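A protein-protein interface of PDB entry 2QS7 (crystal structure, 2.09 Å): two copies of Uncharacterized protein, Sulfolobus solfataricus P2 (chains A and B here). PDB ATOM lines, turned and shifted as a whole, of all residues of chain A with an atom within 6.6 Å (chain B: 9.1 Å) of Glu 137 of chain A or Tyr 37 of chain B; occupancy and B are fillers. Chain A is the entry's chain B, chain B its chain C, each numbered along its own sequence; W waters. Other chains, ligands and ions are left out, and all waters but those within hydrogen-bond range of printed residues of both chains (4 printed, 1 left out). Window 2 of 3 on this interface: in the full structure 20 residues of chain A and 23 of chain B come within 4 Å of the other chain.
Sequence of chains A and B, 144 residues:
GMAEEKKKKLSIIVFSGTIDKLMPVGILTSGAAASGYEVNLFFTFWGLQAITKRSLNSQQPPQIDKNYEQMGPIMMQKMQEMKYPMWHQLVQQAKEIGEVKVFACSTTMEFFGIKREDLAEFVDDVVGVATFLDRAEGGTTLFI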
ATOM      1  N   LYS A   9     -28.789 -16.974  19.872  1.00  0.00           N
ATOM      2  CA  LYS A   9     -28.110 -18.258  19.703  1.00  0.00           C
ATOM      3  C   LYS A   9     -28.358 -19.191  20.867  1.00  0.00           C
ATOM      4  O   LYS A   9     -28.383 -18.755  22.009  1.00  0.00           O
ATOM      5  CB  LYS A   9     -26.615 -17.978  19.544  1.00  0.00           C
ATOM      6  CG  LYS A   9     -25.750 -19.168  19.271  1.00  0.00           C
ATOM      7  CD  LYS A   9     -24.371 -18.762  18.757  1.00  0.00           C
ATOM      8  CE  LYS A   9     -23.639 -17.866  19.703  1.00  0.00           C
ATOM      9  NZ  LYS A   9     -22.282 -17.613  19.178  1.00  0.00           N
ATOM     10  N   SER A  11     -26.961 -23.101  22.114  1.00  0.00           N
ATOM     11  CA  SER A  11     -26.045 -24.192  21.878  1.00  0.00           C
ATOM     12  C   SER A  11     -26.320 -25.213  22.954  1.00  0.00           C
ATOM     13  O   SER A  11     -26.564 -24.859  24.104  1.00  0.00           O
ATOM     14  CB  SER A  11     -24.577 -23.736  21.899  1.00  0.00           C
ATOM     15  OG  SER A  11     -24.398 -22.575  21.064  1.00  0.00           O
ATOM     16  N   ALA A 130     -13.102 -27.259  22.045  1.00  0.00           N
ATOM     17  CA  ALA A 130     -12.792 -25.854  21.869  1.00  0.00           C
ATOM     18  C   ALA A 130     -13.583 -25.217  20.742  1.00  0.00           C
ATOM     19  O   ALA A 130     -14.025 -24.058  20.839  1.00  0.00           O
ATOM     20  CB  ALA A 130     -11.325 -25.688  21.596  1.00  0.00           C
ATOM     21  N   PHE A 132     -16.530 -26.122  19.807  1.00  0.00           N
ATOM     22  CA  PHE A 132     -17.878 -25.878  20.221  1.00  0.00           C
ATOM     23  C   PHE A 132     -17.978 -24.683  21.187  1.00  0.00           C
ATOM     24  O   PHE A 132     -18.892 -23.886  21.049  1.00  0.00           O
ATOM     25  CB  PHE A 132     -18.547 -27.133  20.744  1.00  0.00           C
ATOM     26  CG  PHE A 132     -20.023 -27.052  20.681  1.00  0.00           C
ATOM     27  CD1 PHE A 132     -20.675 -27.227  19.474  1.00  0.00           C
ATOM     28  CD2 PHE A 132     -20.764 -26.753  21.805  1.00  0.00           C
ATOM     29  CE1 PHE A 132     -22.046 -27.131  19.402  1.00  0.00           C
ATOM     30  CE2 PHE A 132     -22.146 -26.649  21.734  1.00  0.00           C
ATOM     31  CZ  PHE A 132     -22.780 -26.842  20.532  1.00  0.00           C
ATOM     32  N   LEU A 133     -17.034 -24.537  22.101  1.00  0.00           N
ATOM     33  CA  LEU A 133     -17.018 -23.395  22.991  1.00  0.00           C
ATOM     34  C   LEU A 133     -17.025 -22.087  22.215  1.00  0.00           C
ATOM     35  O   LEU A 133     -17.713 -21.126  22.568  1.00  0.00           O
ATOM     36  CB  LEU A 133     -15.751 -23.408  23.846  1.00  0.00           C
ATOM     37  CG  LEU A 133     -15.781 -23.880  25.305  1.00  0.00           C
ATOM     38  CD1 LEU A 133     -16.685 -25.039  25.510  1.00  0.00           C
ATOM     39  CD2 LEU A 133     -14.338 -24.169  25.771  1.00  0.00           C
ATOM     40  N   ASP A 134     -16.218 -22.042  21.178  1.00  0.00           N
ATOM     41  CA  ASP A 134     -16.120 -20.864  20.365  1.00  0.00           C
ATOM     42  C   ASP A 134     -17.449 -20.568  19.665  1.00  0.00           C
ATOM     43  O   ASP A 134     -17.869 -19.418  19.593  1.00  0.00           O
ATOM     44  CB  ASP A 134     -14.971 -20.968  19.354  1.00  0.00           C
ATOM     45  CG  ASP A 134     -13.549 -20.942  20.035  1.00  0.00           C
ATOM     46  OD1 ASP A 134     -13.447 -20.760  21.282  1.00  0.00           O
ATOM     47  OD2 ASP A 134     -12.528 -21.107  19.310  1.00  0.00           O
ATOM     48  N   ARG A 135     -18.119 -21.593  19.152  1.00  0.00           N
ATOM     49  CA  ARG A 135     -19.428 -21.368  18.552  1.00  0.00           C
ATOM     50  C   ARG A 135     -20.497 -20.999  19.570  1.00  0.00           C
ATOM     51  O   ARG A 135     -21.396 -20.264  19.230  1.00  0.00           O
ATOM     52  CB  ARG A 135     -19.909 -22.568  17.739  1.00  0.00           C
ATOM     53  CG  ARG A 135     -19.121 -22.765  16.459  1.00  0.00           C
ATOM     54  CD  ARG A 135     -19.858 -23.706  15.537  1.00  0.00           C
ATOM     55  NE  ARG A 135     -21.092 -23.078  15.062  1.00  0.00           N
ATOM     56  CZ  ARG A 135     -21.277 -22.556  13.853  1.00  0.00           C
ATOM     57  NH1 ARG A 135     -20.305 -22.603  12.931  1.00  0.00           N
ATOM     58  NH2 ARG A 135     -22.463 -22.010  13.560  1.00  0.00           N
ATOM     59  N   ALA A 136     -20.421 -21.522  20.790  1.00  0.00           N
ATOM     60  CA  ALA A 136     -21.433 -21.240  21.806  1.00  0.00           C
ATOM     61  C   ALA A 136     -21.323 -19.882  22.439  1.00  0.00           C
ATOM     62  O   ALA A 136     -22.294 -19.355  23.002  1.00  0.00           O
ATOM     63  CB  ALA A 136     -21.369 -22.303  22.908  1.00  0.00           C
ATOM     64  N   GLU A 137     -20.128 -19.327  22.369  1.00  0.00           N
ATOM     65  CA  GLU A 137     -19.803 -18.058  22.991  1.00  0.00           C
ATOM     66  C   GLU A 137     -20.840 -16.966  22.715  1.00  0.00           C
ATOM     67  O   GLU A 137     -21.177 -16.686  21.571  1.00  0.00           O
ATOM     68  CB  GLU A 137     -18.442 -17.599  22.453  1.00  0.00           C
ATOM     69  CG  GLU A 137     -17.907 -16.308  23.029  1.00  0.00           C
ATOM     70  CD  GLU A 137     -17.475 -16.448  24.472  1.00  0.00           C
ATOM     71  OE1 GLU A 137     -17.232 -17.596  24.932  1.00  0.00           O
ATOM     72  OE2 GLU A 137     -17.363 -15.393  25.143  1.00  0.00           O
ATOM     73  N   GLY A 138     -21.326 -16.329  23.768  1.00  0.00           N
ATOM     74  CA  GLY A 138     -22.255 -15.245  23.583  1.00  0.00           C
ATOM     75  C   GLY A 138     -23.738 -15.611  23.552  1.00  0.00           C
ATOM     76  O   GLY A 138     -24.583 -14.741  23.573  1.00  0.00           O
ATOM     77  N   GLY A 139     -24.072 -16.881  23.486  1.00  0.00           N
ATOM     78  CA  GLY A 139     -25.485 -17.260  23.464  1.00  0.00           C
ATOM     79  C   GLY A 139     -25.831 -18.073  24.688  1.00  0.00           C
ATOM     80  O   GLY A 139     -25.039 -18.201  25.582  1.00  0.00           O
ATOM     81  N   THR A 141     -26.334 -21.446  26.584  1.00  0.00           N
ATOM     82  CA  THR A 141     -25.715 -22.766  26.447  1.00  0.00           C
ATOM     83  C   THR A 141     -26.166 -23.695  27.550  1.00  0.00           C
ATOM     84  O   THR A 141     -26.152 -23.336  28.767  1.00  0.00           O
ATOM     85  CB  THR A 141     -24.183 -22.665  26.384  1.00  0.00           C
ATOM     86  OG1 THR A 141     -23.825 -21.667  25.408  1.00  0.00           O
ATOM     87  CG2 THR A 141     -23.521 -24.010  26.007  1.00  0.00           C
ATOM     88  N   LYS B   7     -11.972 -11.825  27.032  1.00  0.00           N
ATOM     89  CA  LYS B   7     -11.722 -12.764  28.177  1.00  0.00           C
ATOM     90  C   LYS B   7     -12.735 -13.925  28.151  1.00  0.00           C
ATOM     91  O   LYS B   7     -13.793 -13.805  28.774  1.00  0.00           O
ATOM     92  CB  LYS B   7     -11.827 -11.995  29.507  1.00  0.00           C
ATOM     93  N   LYS B   8     -12.428 -15.020  27.421  1.00  0.00           N
ATOM     94  CA  LYS B   8     -13.322 -16.148  27.292  1.00  0.00           C
ATOM     95  C   LYS B   8     -13.324 -16.946  28.584  1.00  0.00           C
ATOM     96  O   LYS B   8     -12.280 -17.145  29.198  1.00  0.00           O
ATOM     97  CB  LYS B   8     -12.869 -17.001  26.107  1.00  0.00           C
ATOM     98  CG  LYS B   8     -12.741 -16.260  24.789  1.00  0.00           C
ATOM     99  N   LYS B   9     -14.495 -17.387  29.008  1.00  0.00           N
ATOM    100  CA  LYS B   9     -14.641 -18.035  30.302  1.00  0.00           C
ATOM    101  C   LYS B   9     -15.671 -19.154  30.256  1.00  0.00           C
ATOM    102  O   LYS B   9     -16.714 -19.036  29.576  1.00  0.00           O
ATOM    103  CB  LYS B   9     -15.052 -16.944  31.284  1.00  0.00           C
ATOM    104  CG  LYS B   9     -15.312 -17.379  32.653  1.00  0.00           C
ATOM    105  CD  LYS B   9     -15.434 -16.185  33.603  1.00  0.00           C
ATOM    106  CE  LYS B   9     -16.566 -15.289  33.246  1.00  0.00           C
ATOM    107  NZ  LYS B   9     -16.728 -14.261  34.295  1.00  0.00           N
ATOM    108  N   LEU B  10     -15.348 -20.244  30.944  1.00  0.00           N
ATOM    109  CA  LEU B  10     -16.210 -21.405  31.089  1.00  0.00           C
ATOM    110  C   LEU B  10     -16.314 -21.721  32.560  1.00  0.00           C
ATOM    111  O   LEU B  10     -15.294 -21.838  33.226  1.00  0.00           O
ATOM    112  CB  LEU B  10     -15.598 -22.625  30.395  1.00  0.00           C
ATOM    113  CG  LEU B  10     -16.288 -23.986  30.602  1.00  0.00           C
ATOM    114  CD1 LEU B  10     -17.671 -24.011  30.031  1.00  0.00           C
ATOM    115  CD2 LEU B  10     -15.396 -25.094  29.988  1.00  0.00           C
ATOM    116  N   SER B  11     -17.539 -21.833  33.068  1.00  0.00           N
ATOM    117  CA  SER B  11     -17.759 -22.204  34.464  1.00  0.00           C
ATOM    118  C   SER B  11     -18.662 -23.422  34.468  1.00  0.00           C
ATOM    119  O   SER B  11     -19.591 -23.501  33.683  1.00  0.00           O
ATOM    120  CB  SER B  11     -18.356 -21.031  35.211  1.00  0.00           C
ATOM    121  OG  SER B  11     -17.534 -19.860  35.077  1.00  0.00           O
ATOM    122  N   LEU B  28     -13.678 -30.979  28.925  1.00  0.00           N
ATOM    123  CA  LEU B  28     -14.038 -29.587  28.717  1.00  0.00           C
ATOM    124  C   LEU B  28     -13.002 -28.681  29.347  1.00  0.00           C
ATOM    125  O   LEU B  28     -12.590 -27.702  28.746  1.00  0.00           O
ATOM    126  CB  LEU B  28     -15.420 -29.258  29.325  1.00  0.00           C
ATOM    127  CG  LEU B  28     -16.682 -29.691  28.564  1.00  0.00           C
ATOM    128  CD1 LEU B  28     -17.941 -29.682  29.436  1.00  0.00           C
ATOM    129  CD2 LEU B  28     -16.838 -28.776  27.366  1.00  0.00           C
ATOM    130  N   THR B  29     -12.592 -29.003  30.572  1.00  0.00           N
ATOM    131  CA  THR B  29     -11.627 -28.172  31.294  1.00  0.00           C
ATOM    132  C   THR B  29     -10.310 -28.090  30.559  1.00  0.00           C
ATOM    133  O   THR B  29      -9.786 -27.016  30.326  1.00  0.00           O
ATOM    134  CB  THR B  29     -11.397 -28.658  32.719  1.00  0.00           C
ATOM    135  OG1 THR B  29     -12.633 -28.567  33.431  1.00  0.00           O
ATOM    136  CG2 THR B  29     -10.342 -27.802  33.420  1.00  0.00           C
ATOM    137  N   SER B  30      -9.813 -29.244  30.158  1.00  0.00           N
ATOM    138  CA  SER B  30      -8.553 -29.383  29.459  1.00  0.00           C
ATOM    139  C   SER B  30      -8.562 -28.654  28.127  1.00  0.00           C
ATOM    140  O   SER B  30      -7.666 -27.903  27.813  1.00  0.00           O
ATOM    141  CB  SER B  30      -8.314 -30.869  29.219  1.00  0.00           C
ATOM    142  OG  SER B  30      -7.096 -31.080  28.548  1.00  0.00           O
ATOM    143  N   GLY B  31      -9.590 -28.884  27.332  1.00  0.00           N
ATOM    144  CA  GLY B  31      -9.716 -28.201  26.037  1.00  0.00           C
ATOM    145  C   GLY B  31      -9.897 -26.690  26.178  1.00  0.00           C
ATOM    146  O   GLY B  31      -9.303 -25.907  25.445  1.00  0.00           O
ATOM    147  N   ALA B  32     -10.737 -26.273  27.111  1.00  0.00           N
ATOM    148  CA  ALA B  32     -10.961 -24.856  27.331  1.00  0.00           C
ATOM    149  C   ALA B  32      -9.657 -24.193  27.770  1.00  0.00           C
ATOM    150  O   ALA B  32      -9.252 -23.192  27.184  1.00  0.00           O
ATOM    151  CB  ALA B  32     -12.034 -24.672  28.377  1.00  0.00           C
ATOM    152  N   ALA B  33      -8.980 -24.772  28.768  1.00  0.00           N
ATOM    153  CA  ALA B  33      -7.718 -24.198  29.267  1.00  0.00           C
ATOM    154  C   ALA B  33      -6.700 -24.098  28.150  1.00  0.00           C
ATOM    155  O   ALA B  33      -6.025 -23.079  28.019  1.00  0.00           O
ATOM    156  CB  ALA B  33      -7.142 -24.976  30.437  1.00  0.00           C
ATOM    157  N   ALA B  34      -6.604 -25.138  27.326  1.00  0.00           N
ATOM    158  CA  ALA B  34      -5.651 -25.143  26.216  1.00  0.00           C
ATOM    159  C   ALA B  34      -5.998 -24.051  25.189  1.00  0.00           C
ATOM    160  O   ALA B  34      -5.114 -23.523  24.525  1.00  0.00           O
ATOM    161  CB  ALA B  34      -5.590 -26.534  25.555  1.00  0.00           C
ATOM    162  N   SER B  35      -7.278 -23.718  25.059  1.00  0.00           N
ATOM    163  CA  SER B  35      -7.706 -22.665  24.135  1.00  0.00           C
ATOM    164  C   SER B  35      -7.667 -21.263  24.720  1.00  0.00           C
ATOM    165  O   SER B  35      -8.140 -20.323  24.086  1.00  0.00           O
ATOM    166  CB  SER B  35      -9.104 -22.942  23.622  1.00  0.00           C
ATOM    167  OG  SER B  35      -9.036 -23.988  22.695  1.00  0.00           O
ATOM    168  N   GLY B  36      -7.142 -21.115  25.925  1.00  0.00           N
ATOM    169  CA  GLY B  36      -7.028 -19.795  26.517  1.00  0.00           C
ATOM    170  C   GLY B  36      -8.232 -19.318  27.306  1.00  0.00           C
ATOM    171  O   GLY B  36      -8.325 -18.140  27.609  1.00  0.00           O
ATOM    172  N   TYR B  37      -9.152 -20.222  27.641  1.00  0.00           N
ATOM    173  CA  TYR B  37     -10.291 -19.886  28.487  1.00  0.00           C
ATOM    174  C   TYR B  37      -9.907 -19.893  29.960  1.00  0.00           C
ATOM    175  O   TYR B  37      -9.065 -20.678  30.372  1.00  0.00           O
ATOM    176  CB  TYR B  37     -11.415 -20.918  28.312  1.00  0.00           C
ATOM    177  CG  TYR B  37     -12.256 -20.738  27.095  1.00  0.00           C
ATOM    178  CD1 TYR B  37     -11.735 -20.973  25.831  1.00  0.00           C
ATOM    179  CD2 TYR B  37     -13.580 -20.368  27.203  1.00  0.00           C
ATOM    180  CE1 TYR B  37     -12.501 -20.803  24.700  1.00  0.00           C
ATOM    181  CE2 TYR B  37     -14.363 -20.189  26.083  1.00  0.00           C
ATOM    182  CZ  TYR B  37     -13.820 -20.404  24.833  1.00  0.00           C
ATOM    183  OH  TYR B  37     -14.585 -20.236  23.707  1.00  0.00           O
ATOM    184  N   GLU B  38     -10.529 -19.011  30.728  1.00  0.00           N
ATOM    185  CA  GLU B  38     -10.464 -19.046  32.168  1.00  0.00           C
ATOM    186  C   GLU B  38     -11.548 -20.099  32.493  1.00  0.00           C
ATOM    187  O   GLU B  38     -12.645 -20.075  31.917  1.00  0.00           O
ATOM    188  CB  GLU B  38     -10.793 -17.668  32.722  1.00  0.00           C
ATOM    189  CG  GLU B  38     -10.992 -17.653  34.243  1.00  0.00           C
ATOM    190  CD  GLU B  38     -11.559 -16.307  34.805  1.00  0.00           C
ATOM    191  OE1 GLU B  38     -11.268 -15.215  34.203  1.00  0.00           O
ATOM    192  OE2 GLU B  38     -12.290 -16.395  35.855  1.00  0.00           O
ATOM    193  N   VAL B  39     -11.253 -21.055  33.358  1.00  0.00           N
ATOM    194  CA  VAL B  39     -12.233 -22.084  33.719  1.00  0.00           C
ATOM    195  C   VAL B  39     -12.426 -22.081  35.217  1.00  0.00           C
ATOM    196  O   VAL B  39     -11.470 -22.031  35.961  1.00  0.00           O
ATOM    197  CB  VAL B  39     -11.783 -23.530  33.303  1.00  0.00           C
ATOM    198  CG1 VAL B  39     -12.862 -24.546  33.631  1.00  0.00           C
ATOM    199  CG2 VAL B  39     -11.391 -23.589  31.816  1.00  0.00           C
ATOM    200  N   ASN B  40     -13.683 -22.139  35.630  1.00  0.00           N
ATOM    201  CA  ASN B  40     -14.083 -22.196  37.020  1.00  0.00           C
ATOM    202  C   ASN B  40     -14.925 -23.465  37.215  1.00  0.00           C
ATOM    203  O   ASN B  40     -15.920 -23.663  36.509  1.00  0.00           O
ATOM    204  CB  ASN B  40     -15.020 -21.029  37.362  1.00  0.00           C
ATOM    205  CG  ASN B  40     -14.345 -19.697  37.309  1.00  0.00           C
ATOM    206  OD1 ASN B  40     -13.393 -19.464  38.034  1.00  0.00           O
ATOM    207  ND2 ASN B  40     -14.841 -18.809  36.454  1.00  0.00           N
ATOM    208  N   ALA B  94      -4.639 -29.083  33.423  1.00  0.00           N
ATOM    209  CA  ALA B  94      -5.222 -27.840  32.935  1.00  0.00           C
ATOM    210  C   ALA B  94      -4.810 -26.668  33.837  1.00  0.00           C
ATOM    211  O   ALA B  94      -4.501 -25.587  33.342  1.00  0.00           O
ATOM    212  CB  ALA B  94      -6.719 -27.953  32.875  1.00  0.00           C
ATOM    213  N   LYS B  95      -4.798 -26.874  35.156  1.00  0.00           N
ATOM    214  CA  LYS B  95      -4.375 -25.812  36.084  1.00  0.00           C
ATOM    215  C   LYS B  95      -2.943 -25.366  35.821  1.00  0.00           C
ATOM    216  O   LYS B  95      -2.607 -24.196  35.951  1.00  0.00           O
ATOM    217  CB  LYS B  95      -4.483 -26.242  37.551  1.00  0.00           C
ATOM    218  CG  LYS B  95      -5.900 -26.470  37.993  1.00  0.00           C
ATOM    219  CD  LYS B  95      -6.047 -26.809  39.466  1.00  0.00           C
ATOM    220  CE  LYS B  95      -5.921 -25.593  40.346  1.00  0.00           C
ATOM    221  NZ  LYS B  95      -6.138 -25.977  41.770  1.00  0.00           N
ATOM    222  N   ILE B  97      -1.384 -25.627  32.884  1.00  0.00           N
ATOM    223  CA  ILE B  97      -1.362 -25.018  31.557  1.00  0.00           C
ATOM    224  C   ILE B  97      -2.049 -23.654  31.473  1.00  0.00           C
ATOM    225  O   ILE B  97      -1.543 -22.738  30.833  1.00  0.00           O
ATOM    226  CB  ILE B  97      -2.006 -26.003  30.532  1.00  0.00           C
ATOM    227  CG1 ILE B  97      -0.907 -26.891  29.903  1.00  0.00           C
ATOM    228  CG2 ILE B  97      -2.804 -25.247  29.454  1.00  0.00           C
ATOM    229  CD1 ILE B  97      -0.130 -27.785  30.900  1.00  0.00           C
ATOM    230  N   GLY B  98      -3.206 -23.529  32.109  1.00  0.00           N
ATOM    231  CA  GLY B  98      -3.987 -22.300  32.030  1.00  0.00           C
ATOM    232  C   GLY B  98      -4.517 -21.763  33.343  1.00  0.00           C
ATOM    233  O   GLY B  98      -3.972 -22.034  34.408  1.00  0.00           O
ATOM    234  N   GLU B  99      -5.597 -20.991  33.252  1.00  0.00           N
ATOM    235  CA  GLU B  99      -6.217 -20.361  34.423  1.00  0.00           C
ATOM    236  C   GLU B  99      -7.472 -21.152  34.803  1.00  0.00           C
ATOM    237  O   GLU B  99      -8.557 -20.906  34.289  1.00  0.00           O
ATOM    238  CB  GLU B  99      -6.492 -18.883  34.124  1.00  0.00           C
ATOM    239  CG  GLU B  99      -7.479 -18.134  35.025  1.00  0.00           C
ATOM    240  CD  GLU B  99      -7.027 -17.895  36.460  1.00  0.00           C
ATOM    241  OE1 GLU B  99      -5.848 -17.502  36.664  1.00  0.00           O
ATOM    242  OE2 GLU B  99      -7.893 -18.042  37.378  1.00  0.00           O
ATOM    243  N   VAL B 100      -7.292 -22.128  35.687  1.00  0.00           N
ATOM    244  CA  VAL B 100      -8.360 -23.011  36.126  1.00  0.00           C
ATOM    245  C   VAL B 100      -8.452 -22.934  37.639  1.00  0.00           C
ATOM    246  O   VAL B 100      -7.453 -23.098  38.317  1.00  0.00           O
ATOM    247  CB  VAL B 100      -8.073 -24.476  35.718  1.00  0.00           C
ATOM    248  CG1 VAL B 100      -9.169 -25.426  36.276  1.00  0.00           C
ATOM    249  CG2 VAL B 100      -7.936 -24.578  34.201  1.00  0.00           C
ATOM    250  N   LYS B 101      -9.649 -22.662  38.153  1.00  0.00           N
ATOM    251  CA  LYS B 101      -9.864 -22.594  39.594  1.00  0.00           C
ATOM    252  C   LYS B 101     -10.934 -23.592  39.987  1.00  0.00           C
ATOM    253  O   LYS B 101     -11.988 -23.696  39.348  1.00  0.00           O
ATOM    254  CB  LYS B 101     -10.267 -21.185  40.011  1.00  0.00           C
ATOM    255  CG  LYS B 101      -9.153 -20.175  39.820  1.00  0.00           C
ATOM    256  CD  LYS B 101      -8.092 -20.281  40.889  1.00  0.00           C
ATOM    257  CE  LYS B 101      -6.969 -19.211  40.728  1.00  0.00           C
ATOM    258  NZ  LYS B 101      -6.083 -19.430  39.572  1.00  0.00           N
ATOM    259  N   GLY B 138     -21.201 -13.709  32.696  1.00  0.00           N
ATOM    260  CA  GLY B 138     -20.573 -13.247  31.497  1.00  0.00           C
ATOM    261  C   GLY B 138     -19.919 -14.310  30.644  1.00  0.00           C
ATOM    262  O   GLY B 138     -19.571 -14.033  29.521  1.00  0.00           O
ATOM    263  N   GLY B 139     -19.770 -15.524  31.147  1.00  0.00           N
ATOM    264  CA  GLY B 139     -19.179 -16.589  30.350  1.00  0.00           C
ATOM    265  C   GLY B 139     -20.192 -17.690  30.112  1.00  0.00           C
ATOM    266  O   GLY B 139     -21.370 -17.521  30.398  1.00  0.00           O
ATOM    267  N   THR B 140     -19.723 -18.782  29.529  1.00  0.00           N
ATOM    268  CA  THR B 140     -20.513 -19.958  29.295  1.00  0.00           C
ATOM    269  C   THR B 140     -20.567 -20.724  30.596  1.00  0.00           C
ATOM    270  O   THR B 140     -19.565 -20.919  31.241  1.00  0.00           O
ATOM    271  CB  THR B 140     -19.868 -20.775  28.190  1.00  0.00           C
ATOM    272  OG1 THR B 140     -19.939 -19.995  27.006  1.00  0.00           O
ATOM    273  CG2 THR B 140     -20.573 -22.131  27.993  1.00  0.00           C
ATOM    274  N   THR B 141     -21.764 -21.142  30.989  1.00  0.00           N
ATOM    275  CA  THR B 141     -21.935 -21.826  32.273  1.00  0.00           C
ATOM    276  C   THR B 141     -22.788 -23.063  32.078  1.00  0.00           C
ATOM    277  O   THR B 141     -23.838 -23.016  31.437  1.00  0.00           O
ATOM    278  CB  THR B 141     -22.555 -20.904  33.333  1.00  0.00           C
ATOM    279  OG1 THR B 141     -21.741 -19.721  33.488  1.00  0.00           O
ATOM    280  CG2 THR B 141     -22.691 -21.642  34.702  1.00  0.00           C
HETATM  281  O   HOH W   1     -20.653 -17.091  26.394  1.00  0.00           O
HETATM  282  O   HOH W   2     -22.833 -19.466  26.369  1.00  0.00           O
HETATM  283  O   HOH W   3     -18.096 -20.444  25.158  1.00  0.00           O
HETATM  284  O   HOH W   4     -17.023 -16.651  27.455  1.00  0.00           O
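The side-chain amino group (NZ) of Lys 9 of chain A lies within hydrogen-bond range of the backbone carbonyl oxygen (O) of Glu 137 of chain A, at 2.8 Å. The backbone NH (N) of Ser 11 of chain B is in hydrogen-bond range of the backbone carbonyl oxygen (O) of Thr 140 of chain B (2.9 Å). O of Lys 9 of chain B lies within hydrogen-bond range of N of Thr 140 of chain B, at 3.0 Å. O of Ala 32 of chain B lies within hydrogen-bond range of N of Tyr 37 of chain B. O of Gly 31 of chain B lies within hydrogen-bond range of OG of Ser 35 of chain B.
Among the printed residues, pairs that only touch across the chains: Ala 130 of chain A with Ser 35 of chain B (3.1 Å), Leu 133 of chain A with Ala 32 of chain B (3.5 Å), Glu 137 of chain A with Tyr 37 of chain B (3.9 Å), Thr 141 of chain A with Thr 140 of chain B (3.99 Å) and Thr 141 of chain A with Thr 141 of chain B (3.5 Å).
Of the 29 printed residues of chain B, 5 touch a printed residue of chain A. Of the 12 printed residues of chain A, 5 touch a printed residue of chain B.
Water W2 lies within hydrogen-bond range of the side-chain hydroxyl (OG1) of Thr 141 of chain A, the backbone carbonyl oxygen (O) of Gly 139 of chain A, the side-chain hydroxyl (OG1) of Thr 140 of chain B and the backbone carbonyl oxygen (O) of Ala 136 of chain A. Water W3 lies within hydrogen-bond range of OG1 of Thr 140 of chain B (2.6 Å), O of Leu 133 of chain A (2.7 Å) and OE1 of Glu 137 of chain A (3.0 Å). Water W4 lies within hydrogen-bond range of OE2 of Glu 137 of chain A (2.7 Å) and N of Lys 9 of chain B (3.1 Å). Water W1 lies within hydrogen-bond range of N of Gly 138 of chain A (2.8 Å) and OG1 of Thr 140 of chain B (3.1 Å).
Thr 141 of chain B touches its own counterpart, Thr 141 of chain A. Positions printed for both chains: 9, 11, 138, 139 and 141. Of the 7 pairs that touch across the chains among the printed residues, 1 has its exchanged pair printed and touching as well.
No residue of chain B comes within 4 Å of Ala 136 of chain A. Printed residues of chain B within 4 Å of Glu 137 of chain A: Tyr 37. No residue of chain B comes within 4 Å of Gly 138 of chain A. Gly 139 of chain A touches none of the printed residues of chain B. Of the printed residues of chain B, Thr 141 of chain A touches Thr 140 (3.99 Å) and Thr 141 (3.5 Å). Of the printed residues of chain A, Ala 32 of chain B touches Leu 133. Tyr 37 of chain B touches just these residues of chain A: Leu 133, Asp 134 and Glu 137. Lys 101 of chain B touches none of the printed residues of chain A. Printed residues of chain A within 4 Å of Thr 141 of chain B: Thr 141 (3.5 Å). The nearest residue of chain B that does not touch Glu 137 of chain A is Thr 140 of chain B (4.2 Å).
The side-chain hydroxyl (OH) of Tyr 37 of chain B is in hydrogen-bond range of the side-chain carboxylate (OD1) of Asp 134 of chain A. OH of Tyr 37 of chain B lies close to O of Leu 133 of chain A, at 3.4 Å.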
